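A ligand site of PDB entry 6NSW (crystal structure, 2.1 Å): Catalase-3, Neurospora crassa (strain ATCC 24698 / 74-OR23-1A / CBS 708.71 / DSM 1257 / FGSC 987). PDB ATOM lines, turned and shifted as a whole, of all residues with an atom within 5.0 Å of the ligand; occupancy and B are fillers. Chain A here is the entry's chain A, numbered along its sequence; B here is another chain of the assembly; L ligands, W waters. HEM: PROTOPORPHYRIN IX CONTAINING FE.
O2A of the ligand lies within salt-bridge range of NH1 of Arg 139. FE of the ligand is bound by OH of Tyr 389 (2.2 Å). The guanidinium group (NH1) of Arg 396 is in salt-bridge range of an oxygen (O1D) of the ligand (2.8 Å). The guanidinium group of Arg 99 lies within salt-bridge range of an oxygen (O1A) of the ligand (2.9 Å). NE2 of Gln 393 is in hydrogen-bond range of O1D of the ligand, at 2.8 Å.
The backbone NH (N) of Phe 159 sits at hydrogen-bond distance from the backbone carbonyl oxygen (O) of Gly 174, 2.9 Å away. OG of Ser 388 is in hydrogen-bond range of OD1 of Asp 92 of chain B, at 2.8 Å. NH2 of Arg 385 sits close to OH of Tyr 389. O of Val 173 lies within hydrogen-bond range of NH2 of Arg 385 (3.1 Å). N of Arg 139 is in hydrogen-bond range of O of Ala 160 (3.0 Å). The side-chain amide oxygen (OE1) of Gln 393 is in hydrogen-bond range of the guanidinium group (NH1) of Arg 396 (3.3 Å). The backbone carbonyl oxygen (O) of Asn 175 is in hydrogen-bond range of the backbone NH (N) of Phe 246 (2.9 Å). The backbone carbonyl oxygen (O) of Tyr 389 lies within hydrogen-bond range of the side-chain amide nitrogen (NE2) of Gln 393 (3.1 Å).
Residues that only touch the ligand: Gly 174, Val 101, Phe 365, Phe 188, Val 173, Arg 385, His 102, Asn 175, Ser 388, His 249, Ile 248, Val 100, Leu 381, Gly 158, Thr 392, Phe 159, Phe 180, Ala 185, Leu 88 of chain B and Ala 160. 25 residues have an atom within 4 Å of the ligand: Arg 99, Val 100, Val 101, His 102, Arg 139, Gly 158, Phe 159, Ala 160, Val 173, Gly 174, Asn 175, Phe 180, Ala 185, Phe 188, Ile 248, His 249, Phe 365, Leu 381, Arg 385, Ser 388, Tyr 389, Thr 392, Gln 393, Arg 396 and Leu 88 of chain B. Along chain A the residues within 4 Å of the ligand span positions 99 to 396.
Water W1 lies within hydrogen-bond range of an oxygen (O2A) of the ligand (2.5 Å), the backbone carbonyl oxygen of Arg 139 (2.6 Å) and the side-chain hydroxyl of Ser 141 (2.7 Å). Water W4 lies within hydrogen-bond range of O2D of the ligand (2.5 Å), OG1 of Thr 392 (2.8 Å) and N of Val 100 (3.0 Å). Water W3 bridges N of Phe 365 (2.7 Å) and O1A of the ligand (2.8 Å).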
ATOM      1  N   ARG A  99     -26.477 -21.612 -25.392  1.00  0.00           N
ATOM      2  CA  ARG A  99     -25.597 -22.107 -24.345  1.00  0.00           C
ATOM      3  C   ARG A  99     -24.799 -23.299 -24.859  1.00  0.00           C
ATOM      4  O   ARG A  99     -25.319 -24.142 -25.600  1.00  0.00           O
ATOM      5  CB  ARG A  99     -26.409 -22.515 -23.117  1.00  0.00           C
ATOM      6  CG  ARG A  99     -27.195 -21.382 -22.480  1.00  0.00           C
ATOM      7  CD  ARG A  99     -28.338 -21.918 -21.630  1.00  0.00           C
ATOM      8  NE  ARG A  99     -28.850 -20.901 -20.706  1.00  0.00           N
ATOM      9  CZ  ARG A  99     -29.621 -19.886 -21.058  1.00  0.00           C
ATOM     10  NH1 ARG A  99     -29.990 -19.738 -22.324  1.00  0.00           N
ATOM     11  NH2 ARG A  99     -30.030 -19.014 -20.145  1.00  0.00           N
ATOM     12  N   VAL A 100     -23.519 -23.368 -24.477  1.00  0.00           N
ATOM     13  CA  VAL A 100     -22.661 -24.446 -24.966  1.00  0.00           C
ATOM     14  C   VAL A 100     -23.154 -25.794 -24.460  1.00  0.00           C
ATOM     15  O   VAL A 100     -23.031 -26.809 -25.158  1.00  0.00           O
ATOM     16  CB  VAL A 100     -21.185 -24.180 -24.591  1.00  0.00           C
ATOM     17  CG1 VAL A 100     -20.941 -24.403 -23.115  1.00  0.00           C
ATOM     18  CG2 VAL A 100     -20.256 -25.047 -25.428  1.00  0.00           C
ATOM     19  N   VAL A 101     -23.739 -25.835 -23.267  1.00  0.00           N
ATOM     20  CA  VAL A 101     -24.481 -26.981 -22.757  1.00  0.00           C
ATOM     21  C   VAL A 101     -25.794 -26.459 -22.198  1.00  0.00           C
ATOM     22  O   VAL A 101     -25.930 -25.284 -21.851  1.00  0.00           O
ATOM     23  CB  VAL A 101     -23.705 -27.770 -21.666  1.00  0.00           C
ATOM     24  CG1 VAL A 101     -22.719 -28.725 -22.305  1.00  0.00           C
ATOM     25  CG2 VAL A 101     -22.996 -26.810 -20.734  1.00  0.00           C
ATOM     26  N   HIS A 102     -26.776 -27.352 -22.108  1.00  0.00           N
ATOM     27  CA  HIS A 102     -28.108 -27.007 -21.603  1.00  0.00           C
ATOM     28  C   HIS A 102     -28.787 -25.948 -22.472  1.00  0.00           C
ATOM     29  O   HIS A 102     -29.502 -25.077 -21.972  1.00  0.00           O
ATOM     30  CB  HIS A 102     -28.058 -26.527 -20.150  1.00  0.00           C
ATOM     31  CG  HIS A 102     -27.521 -27.530 -19.174  1.00  0.00           C
ATOM     32  ND1 HIS A 102     -28.322 -28.122 -18.214  1.00  0.00           N
ATOM     33  CD2 HIS A 102     -26.279 -28.021 -18.985  1.00  0.00           C
ATOM     34  CE1 HIS A 102     -27.576 -28.946 -17.491  1.00  0.00           C
ATOM     35  NE2 HIS A 102     -26.339 -28.900 -17.940  1.00  0.00           N
ATOM     36  N   ARG A 139     -34.419 -22.036 -14.193  1.00  0.00           N
ATOM     37  CA  ARG A 139     -34.418 -22.546 -15.550  1.00  0.00           C
ATOM     38  C   ARG A 139     -34.157 -24.047 -15.508  1.00  0.00           C
ATOM     39  O   ARG A 139     -33.181 -24.499 -14.905  1.00  0.00           O
ATOM     40  CB  ARG A 139     -33.366 -21.845 -16.425  1.00  0.00           C
ATOM     41  CG  ARG A 139     -33.367 -22.275 -17.889  1.00  0.00           C
ATOM     42  CD  ARG A 139     -32.449 -21.385 -18.715  1.00  0.00           C
ATOM     43  NE  ARG A 139     -32.539 -21.628 -20.157  1.00  0.00           N
ATOM     44  CZ  ARG A 139     -31.940 -22.631 -20.785  1.00  0.00           C
ATOM     45  NH1 ARG A 139     -31.199 -23.498 -20.103  1.00  0.00           N
ATOM     46  NH2 ARG A 139     -32.073 -22.773 -22.093  1.00  0.00           N
ATOM     47  N   SER A 141     -33.737 -27.611 -17.978  1.00  0.00           N
ATOM     48  CA  SER A 141     -33.113 -27.826 -19.272  1.00  0.00           C
ATOM     49  C   SER A 141     -32.750 -29.290 -19.452  1.00  0.00           C
ATOM     50  O   SER A 141     -32.785 -30.082 -18.503  1.00  0.00           O
ATOM     51  CB  SER A 141     -31.861 -26.947 -19.419  1.00  0.00           C
ATOM     52  OG  SER A 141     -30.954 -27.178 -18.352  1.00  0.00           O
ATOM     53  N   GLY A 158     -31.074 -30.093 -16.355  1.00  0.00           N
ATOM     54  CA  GLY A 158     -30.636 -28.990 -15.530  1.00  0.00           C
ATOM     55  C   GLY A 158     -31.756 -28.452 -14.645  1.00  0.00           C
ATOM     56  O   GLY A 158     -32.938 -28.559 -14.968  1.00  0.00           O
ATOM     57  N   PHE A 159     -31.352 -27.867 -13.515  1.00  0.00           N
ATOM     58  CA  PHE A 159     -32.236 -27.368 -12.462  1.00  0.00           C
ATOM     59  C   PHE A 159     -31.482 -26.233 -11.786  1.00  0.00           C
ATOM     60  O   PHE A 159     -30.882 -26.383 -10.718  1.00  0.00           O
ATOM     61  CB  PHE A 159     -32.620 -28.488 -11.480  1.00  0.00           C
ATOM     62  CG  PHE A 159     -33.790 -28.178 -10.586  1.00  0.00           C
ATOM     63  CD1 PHE A 159     -34.098 -26.878 -10.207  1.00  0.00           C
ATOM     64  CD2 PHE A 159     -34.571 -29.209 -10.093  1.00  0.00           C
ATOM     65  CE1 PHE A 159     -35.172 -26.614  -9.364  1.00  0.00           C
ATOM     66  CE2 PHE A 159     -35.650 -28.955  -9.257  1.00  0.00           C
ATOM     67  CZ  PHE A 159     -35.943 -27.655  -8.888  1.00  0.00           C
ATOM     68  N   ALA A 160     -31.491 -25.070 -12.429  1.00  0.00           N
ATOM     69  CA  ALA A 160     -30.708 -23.921 -11.994  1.00  0.00           C
ATOM     70  C   ALA A 160     -31.613 -22.904 -11.313  1.00  0.00           C
ATOM     71  O   ALA A 160     -32.592 -22.437 -11.911  1.00  0.00           O
ATOM     72  CB  ALA A 160     -29.973 -23.275 -13.163  1.00  0.00           C
ATOM     73  N   VAL A 173     -26.646 -23.968  -9.285  1.00  0.00           N
ATOM     74  CA  VAL A 173     -26.712 -24.458 -10.664  1.00  0.00           C
ATOM     75  C   VAL A 173     -26.651 -25.977 -10.582  1.00  0.00           C
ATOM     76  O   VAL A 173     -25.577 -26.581 -10.554  1.00  0.00           O
ATOM     77  CB  VAL A 173     -25.606 -23.873 -11.532  1.00  0.00           C
ATOM     78  CG1 VAL A 173     -25.828 -24.225 -12.996  1.00  0.00           C
ATOM     79  CG2 VAL A 173     -25.512 -22.360 -11.347  1.00  0.00           C
ATOM     80  N   GLY A 174     -27.825 -26.608 -10.543  1.00  0.00           N
ATOM     81  CA  GLY A 174     -27.926 -28.015 -10.278  1.00  0.00           C
ATOM     82  C   GLY A 174     -28.463 -28.827 -11.448  1.00  0.00           C
ATOM     83  O   GLY A 174     -28.709 -28.338 -12.542  1.00  0.00           O
ATOM     84  N   ASN A 175     -28.626 -30.119 -11.170  1.00  0.00           N
ATOM     85  CA  ASN A 175     -29.223 -31.061 -12.097  1.00  0.00           C
ATOM     86  C   ASN A 175     -30.249 -31.887 -11.351  1.00  0.00           C
ATOM     87  O   ASN A 175     -30.304 -31.888 -10.122  1.00  0.00           O
ATOM     88  CB  ASN A 175     -28.158 -31.975 -12.742  1.00  0.00           C
ATOM     89  CG  ASN A 175     -27.357 -31.271 -13.828  1.00  0.00           C
ATOM     90  OD1 ASN A 175     -27.800 -30.275 -14.407  1.00  0.00           O
ATOM     91  ND2 ASN A 175     -26.169 -31.790 -14.117  1.00  0.00           N
ATOM     92  N   PHE A 180     -22.330 -36.518 -11.090  1.00  0.00           N
ATOM     93  CA  PHE A 180     -21.922 -36.108 -12.428  1.00  0.00           C
ATOM     94  C   PHE A 180     -20.931 -37.105 -13.013  1.00  0.00           C
ATOM     95  O   PHE A 180     -20.354 -37.943 -12.301  1.00  0.00           O
ATOM     96  CB  PHE A 180     -21.313 -34.710 -12.436  1.00  0.00           C
ATOM     97  CG  PHE A 180     -21.409 -34.032 -13.771  1.00  0.00           C
ATOM     98  CD1 PHE A 180     -22.642 -33.656 -14.270  1.00  0.00           C
ATOM     99  CD2 PHE A 180     -20.284 -33.837 -14.555  1.00  0.00           C
ATOM    100  CE1 PHE A 180     -22.757 -33.057 -15.509  1.00  0.00           C
ATOM    101  CE2 PHE A 180     -20.385 -33.236 -15.794  1.00  0.00           C
ATOM    102  CZ  PHE A 180     -21.620 -32.854 -16.274  1.00  0.00           C
ATOM    103  N   ALA A 185     -12.760 -30.955 -13.734  1.00  0.00           N
ATOM    104  CA  ALA A 185     -13.412 -30.077 -14.694  1.00  0.00           C
ATOM    105  C   ALA A 185     -12.672 -30.032 -16.022  1.00  0.00           C
ATOM    106  O   ALA A 185     -13.287 -29.790 -17.077  1.00  0.00           O
ATOM    107  CB  ALA A 185     -13.538 -28.668 -14.122  1.00  0.00           C
ATOM    108  N   PHE A 188     -14.287 -31.814 -18.905  1.00  0.00           N
ATOM    109  CA  PHE A 188     -15.624 -31.470 -19.383  1.00  0.00           C
ATOM    110  C   PHE A 188     -15.720 -31.393 -20.898  1.00  0.00           C
ATOM    111  O   PHE A 188     -16.701 -31.922 -21.457  1.00  0.00           O
ATOM    112  CB  PHE A 188     -16.089 -30.154 -18.730  1.00  0.00           C
ATOM    113  CG  PHE A 188     -17.554 -29.884 -18.895  1.00  0.00           C
ATOM    114  CD1 PHE A 188     -18.500 -30.722 -18.326  1.00  0.00           C
ATOM    115  CD2 PHE A 188     -17.996 -28.779 -19.610  1.00  0.00           C
ATOM    116  CE1 PHE A 188     -19.854 -30.478 -18.463  1.00  0.00           C
ATOM    117  CE2 PHE A 188     -19.343 -28.531 -19.758  1.00  0.00           C
ATOM    118  CZ  PHE A 188     -20.275 -29.367 -19.188  1.00  0.00           C
ATOM    119  N   PHE A 246     -30.522 -31.180  -7.368  1.00  0.00           N
ATOM    120  CA  PHE A 246     -29.301 -31.453  -6.619  1.00  0.00           C
ATOM    121  C   PHE A 246     -28.233 -30.447  -6.995  1.00  0.00           C
ATOM    122  O   PHE A 246     -28.007 -30.186  -8.191  1.00  0.00           O
ATOM    123  CB  PHE A 246     -28.785 -32.862  -6.895  1.00  0.00           C
ATOM    124  CG  PHE A 246     -29.786 -33.945  -6.636  1.00  0.00           C
ATOM    125  CD1 PHE A 246     -29.900 -34.505  -5.375  1.00  0.00           C
ATOM    126  CD2 PHE A 246     -30.619 -34.394  -7.644  1.00  0.00           C
ATOM    127  CE1 PHE A 246     -30.828 -35.505  -5.124  1.00  0.00           C
ATOM    128  CE2 PHE A 246     -31.554 -35.391  -7.404  1.00  0.00           C
ATOM    129  CZ  PHE A 246     -31.654 -35.949  -6.143  1.00  0.00           C
ATOM    130  N   GLY A 247     -27.556 -29.882  -5.993  1.00  0.00           N
ATOM    131  CA  GLY A 247     -26.349 -29.136  -6.262  1.00  0.00           C
ATOM    132  C   GLY A 247     -25.171 -30.018  -6.613  1.00  0.00           C
ATOM    133  O   GLY A 247     -24.189 -29.529  -7.192  1.00  0.00           O
ATOM    134  N   ILE A 248     -25.250 -31.310  -6.275  1.00  0.00           N
ATOM    135  CA  ILE A 248     -24.258 -32.342  -6.558  1.00  0.00           C
ATOM    136  C   ILE A 248     -23.003 -32.149  -5.721  1.00  0.00           C
ATOM    137  O   ILE A 248     -22.658 -33.003  -4.898  1.00  0.00           O
ATOM    138  CB  ILE A 248     -23.915 -32.416  -8.053  1.00  0.00           C
ATOM    139  CG1 ILE A 248     -25.180 -32.686  -8.868  1.00  0.00           C
ATOM    140  CG2 ILE A 248     -22.860 -33.489  -8.307  1.00  0.00           C
ATOM    141  CD1 ILE A 248     -24.915 -32.947 -10.327  1.00  0.00           C
ATOM    142  N   HIS A 249     -22.297 -31.033  -5.921  1.00  0.00           N
ATOM    143  CA  HIS A 249     -21.078 -30.781  -5.167  1.00  0.00           C
ATOM    144  C   HIS A 249     -21.365 -30.650  -3.683  1.00  0.00           C
ATOM    145  O   HIS A 249     -22.433 -30.193  -3.261  1.00  0.00           O
ATOM    146  CB  HIS A 249     -20.388 -29.499  -5.647  1.00  0.00           C
ATOM    147  CG  HIS A 249     -20.031 -29.495  -7.090  1.00  0.00           C
ATOM    148  ND1 HIS A 249     -19.250 -30.484  -7.665  1.00  0.00           N
ATOM    149  CD2 HIS A 249     -20.335 -28.635  -8.088  1.00  0.00           C
ATOM    150  CE1 HIS A 249     -19.099 -30.225  -8.950  1.00  0.00           C
ATOM    151  NE2 HIS A 249     -19.745 -29.111  -9.236  1.00  0.00           N
ATOM    152  N   ILE A 363     -30.607 -15.106 -19.336  1.00  0.00           N
ATOM    153  CA  ILE A 363     -30.128 -15.248 -17.957  1.00  0.00           C
ATOM    154  C   ILE A 363     -28.841 -16.055 -17.944  1.00  0.00           C
ATOM    155  O   ILE A 363     -28.674 -17.016 -18.706  1.00  0.00           O
ATOM    156  CB  ILE A 363     -31.203 -15.861 -17.047  1.00  0.00           C
ATOM    157  CG1 ILE A 363     -30.774 -15.768 -15.584  1.00  0.00           C
ATOM    158  CG2 ILE A 363     -31.500 -17.316 -17.433  1.00  0.00           C
ATOM    159  CD1 ILE A 363     -31.878 -16.007 -14.586  1.00  0.00           C
ATOM    160  N   SER A 364     -27.909 -15.650 -17.082  1.00  0.00           N
ATOM    161  CA  SER A 364     -26.547 -16.176 -17.041  1.00  0.00           C
ATOM    162  C   SER A 364     -26.267 -16.724 -15.644  1.00  0.00           C
ATOM    163  O   SER A 364     -25.898 -15.958 -14.738  1.00  0.00           O
ATOM    164  CB  SER A 364     -25.544 -15.081 -17.408  1.00  0.00           C
ATOM    165  OG  SER A 364     -25.749 -14.611 -18.733  1.00  0.00           O
ATOM    166  N   PHE A 365     -26.424 -18.031 -15.466  1.00  0.00           N
ATOM    167  CA  PHE A 365     -26.146 -18.669 -14.190  1.00  0.00           C
ATOM    168  C   PHE A 365     -24.642 -18.876 -14.009  1.00  0.00           C
ATOM    169  O   PHE A 365     -23.900 -19.057 -14.979  1.00  0.00           O
ATOM    170  CB  PHE A 365     -26.869 -20.009 -14.083  1.00  0.00           C
ATOM    171  CG  PHE A 365     -28.351 -19.898 -13.879  1.00  0.00           C
ATOM    172  CD1 PHE A 365     -28.877 -19.661 -12.614  1.00  0.00           C
ATOM    173  CD2 PHE A 365     -29.223 -20.012 -14.946  1.00  0.00           C
ATOM    174  CE1 PHE A 365     -30.250 -19.558 -12.419  1.00  0.00           C
ATOM    175  CE2 PHE A 365     -30.597 -19.899 -14.764  1.00  0.00           C
ATOM    176  CZ  PHE A 365     -31.106 -19.676 -13.504  1.00  0.00           C
ATOM    177  N   LEU A 381     -14.182 -30.790  -9.799  1.00  0.00           N
ATOM    178  CA  LEU A 381     -15.148 -30.469 -10.833  1.00  0.00           C
ATOM    179  C   LEU A 381     -15.759 -29.086 -10.599  1.00  0.00           C
ATOM    180  O   LEU A 381     -15.869 -28.282 -11.532  1.00  0.00           O
ATOM    181  CB  LEU A 381     -16.248 -31.530 -10.871  1.00  0.00           C
ATOM    182  CG  LEU A 381     -17.179 -31.556 -12.084  1.00  0.00           C
ATOM    183  CD1 LEU A 381     -16.434 -32.087 -13.296  1.00  0.00           C
ATOM    184  CD2 LEU A 381     -18.415 -32.389 -11.793  1.00  0.00           C
ATOM    185  N   GLY A 384     -13.250 -25.951 -11.501  1.00  0.00           N
ATOM    186  CA  GLY A 384     -13.145 -25.442 -12.852  1.00  0.00           C
ATOM    187  C   GLY A 384     -14.422 -24.803 -13.348  1.00  0.00           C
ATOM    188  O   GLY A 384     -14.375 -23.924 -14.216  1.00  0.00           O
ATOM    189  N   ARG A 385     -15.578 -25.224 -12.825  1.00  0.00           N
ATOM    190  CA  ARG A 385     -16.831 -24.552 -13.151  1.00  0.00           C
ATOM    191  C   ARG A 385     -16.744 -23.062 -12.866  1.00  0.00           C
ATOM    192  O   ARG A 385     -17.192 -22.242 -13.676  1.00  0.00           O
ATOM    193  CB  ARG A 385     -17.984 -25.184 -12.367  1.00  0.00           C
ATOM    194  CG  ARG A 385     -18.357 -26.588 -12.838  1.00  0.00           C
ATOM    195  CD  ARG A 385     -19.533 -27.167 -12.061  1.00  0.00           C
ATOM    196  NE  ARG A 385     -20.794 -26.556 -12.464  1.00  0.00           N
ATOM    197  CZ  ARG A 385     -21.880 -26.504 -11.696  1.00  0.00           C
ATOM    198  NH1 ARG A 385     -21.848 -27.031 -10.474  1.00  0.00           N
ATOM    199  NH2 ARG A 385     -22.992 -25.924 -12.129  1.00  0.00           N
ATOM    200  N   SER A 388     -15.324 -21.429 -15.725  1.00  0.00           N
ATOM    201  CA  SER A 388     -15.940 -21.689 -17.031  1.00  0.00           C
ATOM    202  C   SER A 388     -17.220 -20.881 -17.242  1.00  0.00           C
ATOM    203  O   SER A 388     -17.478 -20.400 -18.355  1.00  0.00           O
ATOM    204  CB  SER A 388     -16.211 -23.185 -17.173  1.00  0.00           C
ATOM    205  OG  SER A 388     -17.115 -23.451 -18.230  1.00  0.00           O
ATOM    206  N   TYR A 389     -18.041 -20.713 -16.202  1.00  0.00           N
ATOM    207  CA  TYR A 389     -19.320 -20.009 -16.362  1.00  0.00           C
ATOM    208  C   TYR A 389     -19.141 -18.504 -16.491  1.00  0.00           C
ATOM    209  O   TYR A 389     -19.910 -17.848 -17.188  1.00  0.00           O
ATOM    210  CB  TYR A 389     -20.246 -20.280 -15.193  1.00  0.00           C
ATOM    211  CG  TYR A 389     -20.742 -21.699 -15.064  1.00  0.00           C
ATOM    212  CD1 TYR A 389     -19.913 -22.704 -14.584  1.00  0.00           C
ATOM    213  CD2 TYR A 389     -22.069 -22.019 -15.348  1.00  0.00           C
ATOM    214  CE1 TYR A 389     -20.354 -23.979 -14.429  1.00  0.00           C
ATOM    215  CE2 TYR A 389     -22.527 -23.321 -15.197  1.00  0.00           C
ATOM    216  CZ  TYR A 389     -21.668 -24.289 -14.736  1.00  0.00           C
ATOM    217  OH  TYR A 389     -22.124 -25.561 -14.562  1.00  0.00           O
ATOM    218  N   THR A 392     -17.703 -18.101 -20.287  1.00  0.00           N
ATOM    219  CA  THR A 392     -18.596 -18.379 -21.413  1.00  0.00           C
ATOM    220  C   THR A 392     -19.631 -17.273 -21.626  1.00  0.00           C
ATOM    221  O   THR A 392     -20.166 -17.156 -22.741  1.00  0.00           O
ATOM    222  CB  THR A 392     -19.308 -19.719 -21.210  1.00  0.00           C
ATOM    223  OG1 THR A 392     -19.836 -20.173 -22.462  1.00  0.00           O
ATOM    224  CG2 THR A 392     -20.445 -19.586 -20.199  1.00  0.00           C
ATOM    225  N   GLN A 393     -19.927 -16.462 -20.602  1.00  0.00           N
ATOM    226  CA  GLN A 393     -20.823 -15.330 -20.801  1.00  0.00           C
ATOM    227  C   GLN A 393     -20.251 -14.344 -21.801  1.00  0.00           C
ATOM    228  O   GLN A 393     -21.004 -13.696 -22.535  1.00  0.00           O
ATOM    229  CB  GLN A 393     -21.085 -14.626 -19.461  1.00  0.00           C
ATOM    230  CG  GLN A 393     -21.893 -15.410 -18.415  1.00  0.00           C
ATOM    231  CD  GLN A 393     -22.816 -16.460 -18.995  1.00  0.00           C
ATOM    232  OE1 GLN A 393     -23.705 -16.144 -19.791  1.00  0.00           O
ATOM    233  NE2 GLN A 393     -22.624 -17.716 -18.602  1.00  0.00           N
ATOM    234  N   ARG A 396     -21.532 -15.694 -24.979  1.00  0.00           N
ATOM    235  CA  ARG A 396     -22.974 -15.635 -25.216  1.00  0.00           C
ATOM    236  C   ARG A 396     -23.472 -14.198 -25.322  1.00  0.00           C
ATOM    237  O   ARG A 396     -24.371 -13.911 -26.111  1.00  0.00           O
ATOM    238  CB  ARG A 396     -23.711 -16.384 -24.111  1.00  0.00           C
ATOM    239  CG  ARG A 396     -25.020 -16.989 -24.582  1.00  0.00           C
ATOM    240  CD  ARG A 396     -25.290 -18.331 -23.923  1.00  0.00           C
ATOM    241  NE  ARG A 396     -25.438 -18.212 -22.476  1.00  0.00           N
ATOM    242  CZ  ARG A 396     -26.502 -17.692 -21.873  1.00  0.00           C
ATOM    243  NH1 ARG A 396     -26.542 -17.630 -20.547  1.00  0.00           N
ATOM    244  NH2 ARG A 396     -27.524 -17.240 -22.575  1.00  0.00           N
ATOM    245  N   LEU B  88     -10.351 -24.926 -21.548  1.00  0.00           N
ATOM    246  CA  LEU B  88     -11.742 -24.615 -21.227  1.00  0.00           C
ATOM    247  C   LEU B  88     -12.208 -23.328 -21.893  1.00  0.00           C
ATOM    248  O   LEU B  88     -13.393 -23.200 -22.201  1.00  0.00           O
ATOM    249  CB  LEU B  88     -11.936 -24.535 -19.710  1.00  0.00           C
ATOM    250  CG  LEU B  88     -12.529 -25.791 -19.072  1.00  0.00           C
ATOM    251  CD1 LEU B  88     -13.891 -26.121 -19.691  1.00  0.00           C
ATOM    252  CD2 LEU B  88     -11.588 -26.981 -19.209  1.00  0.00           C
ATOM    253  N   PHE B  91     -13.400 -24.338 -25.298  1.00  0.00           N
ATOM    254  CA  PHE B  91     -14.688 -25.000 -25.155  1.00  0.00           C
ATOM    255  C   PHE B  91     -15.790 -24.002 -24.831  1.00  0.00           C
ATOM    256  O   PHE B  91     -16.879 -24.047 -25.414  1.00  0.00           O
ATOM    257  CB  PHE B  91     -14.622 -26.082 -24.082  1.00  0.00           C
ATOM    258  CG  PHE B  91     -15.974 -26.631 -23.706  1.00  0.00           C
ATOM    259  CD1 PHE B  91     -16.595 -27.589 -24.506  1.00  0.00           C
ATOM    260  CD2 PHE B  91     -16.646 -26.175 -22.580  1.00  0.00           C
ATOM    261  CE1 PHE B  91     -17.845 -28.085 -24.178  1.00  0.00           C
ATOM    262  CE2 PHE B  91     -17.896 -26.670 -22.253  1.00  0.00           C
ATOM    263  CZ  PHE B  91     -18.489 -27.624 -23.051  1.00  0.00           C
ATOM    264  N   ASP B  92     -15.527 -23.083 -23.884  1.00  0.00           N
ATOM    265  CA  ASP B  92     -16.542 -22.111 -23.492  1.00  0.00           C
ATOM    266  C   ASP B  92     -16.995 -21.224 -24.647  1.00  0.00           C
ATOM    267  O   ASP B  92     -18.069 -20.606 -24.554  1.00  0.00           O
ATOM    268  CB  ASP B  92     -16.032 -21.211 -22.362  1.00  0.00           C
ATOM    269  CG  ASP B  92     -15.745 -21.955 -21.075  1.00  0.00           C
ATOM    270  OD1 ASP B  92     -16.285 -23.070 -20.881  1.00  0.00           O
ATOM    271  OD2 ASP B  92     -14.975 -21.423 -20.253  1.00  0.00           O
HETATM  272  CHA HEM L   1     -24.636 -24.763 -18.065  1.00  0.00           C
HETATM  273  CHB HEM L   1     -25.344 -27.752 -14.300  1.00  0.00           C
HETATM  274  CHC HEM L   1     -20.784 -29.321 -14.804  1.00  0.00           C
HETATM  275  CHD HEM L   1     -19.876 -25.673 -17.856  1.00  0.00           C
HETATM  276  C1A HEM L   1     -25.243 -25.462 -17.037  1.00  0.00           C
HETATM  277  C2A HEM L   1     -26.640 -25.389 -16.657  1.00  0.00           C
HETATM  278  C3A HEM L   1     -26.831 -26.211 -15.630  1.00  0.00           C
HETATM  279  C4A HEM L   1     -25.571 -26.838 -15.306  1.00  0.00           C
HETATM  280  CMA HEM L   1     -28.181 -26.454 -14.914  1.00  0.00           C
HETATM  281  CAA HEM L   1     -27.723 -24.529 -17.336  1.00  0.00           C
HETATM  282  CBA HEM L   1     -27.969 -23.219 -16.589  1.00  0.00           C
HETATM  283  CGA HEM L   1     -29.117 -22.531 -17.287  1.00  0.00           C
HETATM  284  O1A HEM L   1     -28.906 -21.449 -17.886  1.00  0.00           O
HETATM  285  O2A HEM L   1     -30.236 -23.102 -17.249  1.00  0.00           O
HETATM  286  C1B HEM L   1     -24.155 -28.408 -14.058  1.00  0.00           C
HETATM  287  C2B HEM L   1     -23.864 -29.269 -12.935  1.00  0.00           C
HETATM  288  C3B HEM L   1     -22.594 -29.714 -13.071  1.00  0.00           C
HETATM  289  C4B HEM L   1     -22.054 -29.135 -14.290  1.00  0.00           C
HETATM  290  CMB HEM L   1     -24.889 -29.579 -11.816  1.00  0.00           C
HETATM  291  CAB HEM L   1     -21.765 -30.647 -12.163  1.00  0.00           C
HETATM  292  CBB HEM L   1     -22.107 -31.001 -10.920  1.00  0.00           C
HETATM  293  C1C HEM L   1     -20.106 -28.419 -15.593  1.00  0.00           C
HETATM  294  C2C HEM L   1     -18.669 -28.309 -15.761  1.00  0.00           C
HETATM  295  C3C HEM L   1     -18.428 -27.307 -16.616  1.00  0.00           C
HETATM  296  C4C HEM L   1     -19.698 -26.737 -16.998  1.00  0.00           C
HETATM  297  CMC HEM L   1     -17.658 -29.250 -15.065  1.00  0.00           C
HETATM  298  CAC HEM L   1     -17.074 -26.742 -17.133  1.00  0.00           C
HETATM  299  CBC HEM L   1     -15.908 -26.912 -16.512  1.00  0.00           C
HETATM  300  C1D HEM L   1     -21.083 -25.101 -18.190  1.00  0.00           C
HETATM  301  C2D HEM L   1     -21.285 -24.007 -19.111  1.00  0.00           C
HETATM  302  C3D HEM L   1     -22.588 -23.745 -19.165  1.00  0.00           C
HETATM  303  C4D HEM L   1     -23.273 -24.673 -18.286  1.00  0.00           C
HETATM  304  CMD HEM L   1     -20.152 -23.264 -19.866  1.00  0.00           C
HETATM  305  CAD HEM L   1     -23.232 -22.637 -20.035  1.00  0.00           C
HETATM  306  CBD HEM L   1     -23.661 -21.473 -19.136  1.00  0.00           C
HETATM  307  CGD HEM L   1     -24.129 -20.310 -19.964  1.00  0.00           C
HETATM  308  O1D HEM L   1     -24.717 -19.361 -19.372  1.00  0.00           O
HETATM  309  O2D HEM L   1     -23.929 -20.308 -21.212  1.00  0.00           O
HETATM  310  NA  HEM L   1     -24.625 -26.364 -16.188  1.00  0.00           N
HETATM  311  NB  HEM L   1     -23.030 -28.344 -14.856  1.00  0.00           N
HETATM  312  NC  HEM L   1     -20.698 -27.428 -16.361  1.00  0.00           N
HETATM  313  ND  HEM L   1     -22.314 -25.488 -17.714  1.00  0.00           N
HETATM  314 FE   HEM L   1     -22.657 -26.928 -16.259  1.00  0.00          FE
HETATM  315  O   HOH W   1     -31.330 -25.253 -16.500  1.00  0.00           O
HETATM  316  O   HOH W   2     -24.083 -30.323 -17.173  1.00  0.00           O
HETATM  317  O   HOH W   3     -26.674 -19.861 -17.474  1.00  0.00           O
HETATM  318  O   HOH W   4     -22.424 -20.931 -23.157  1.00  0.00           O
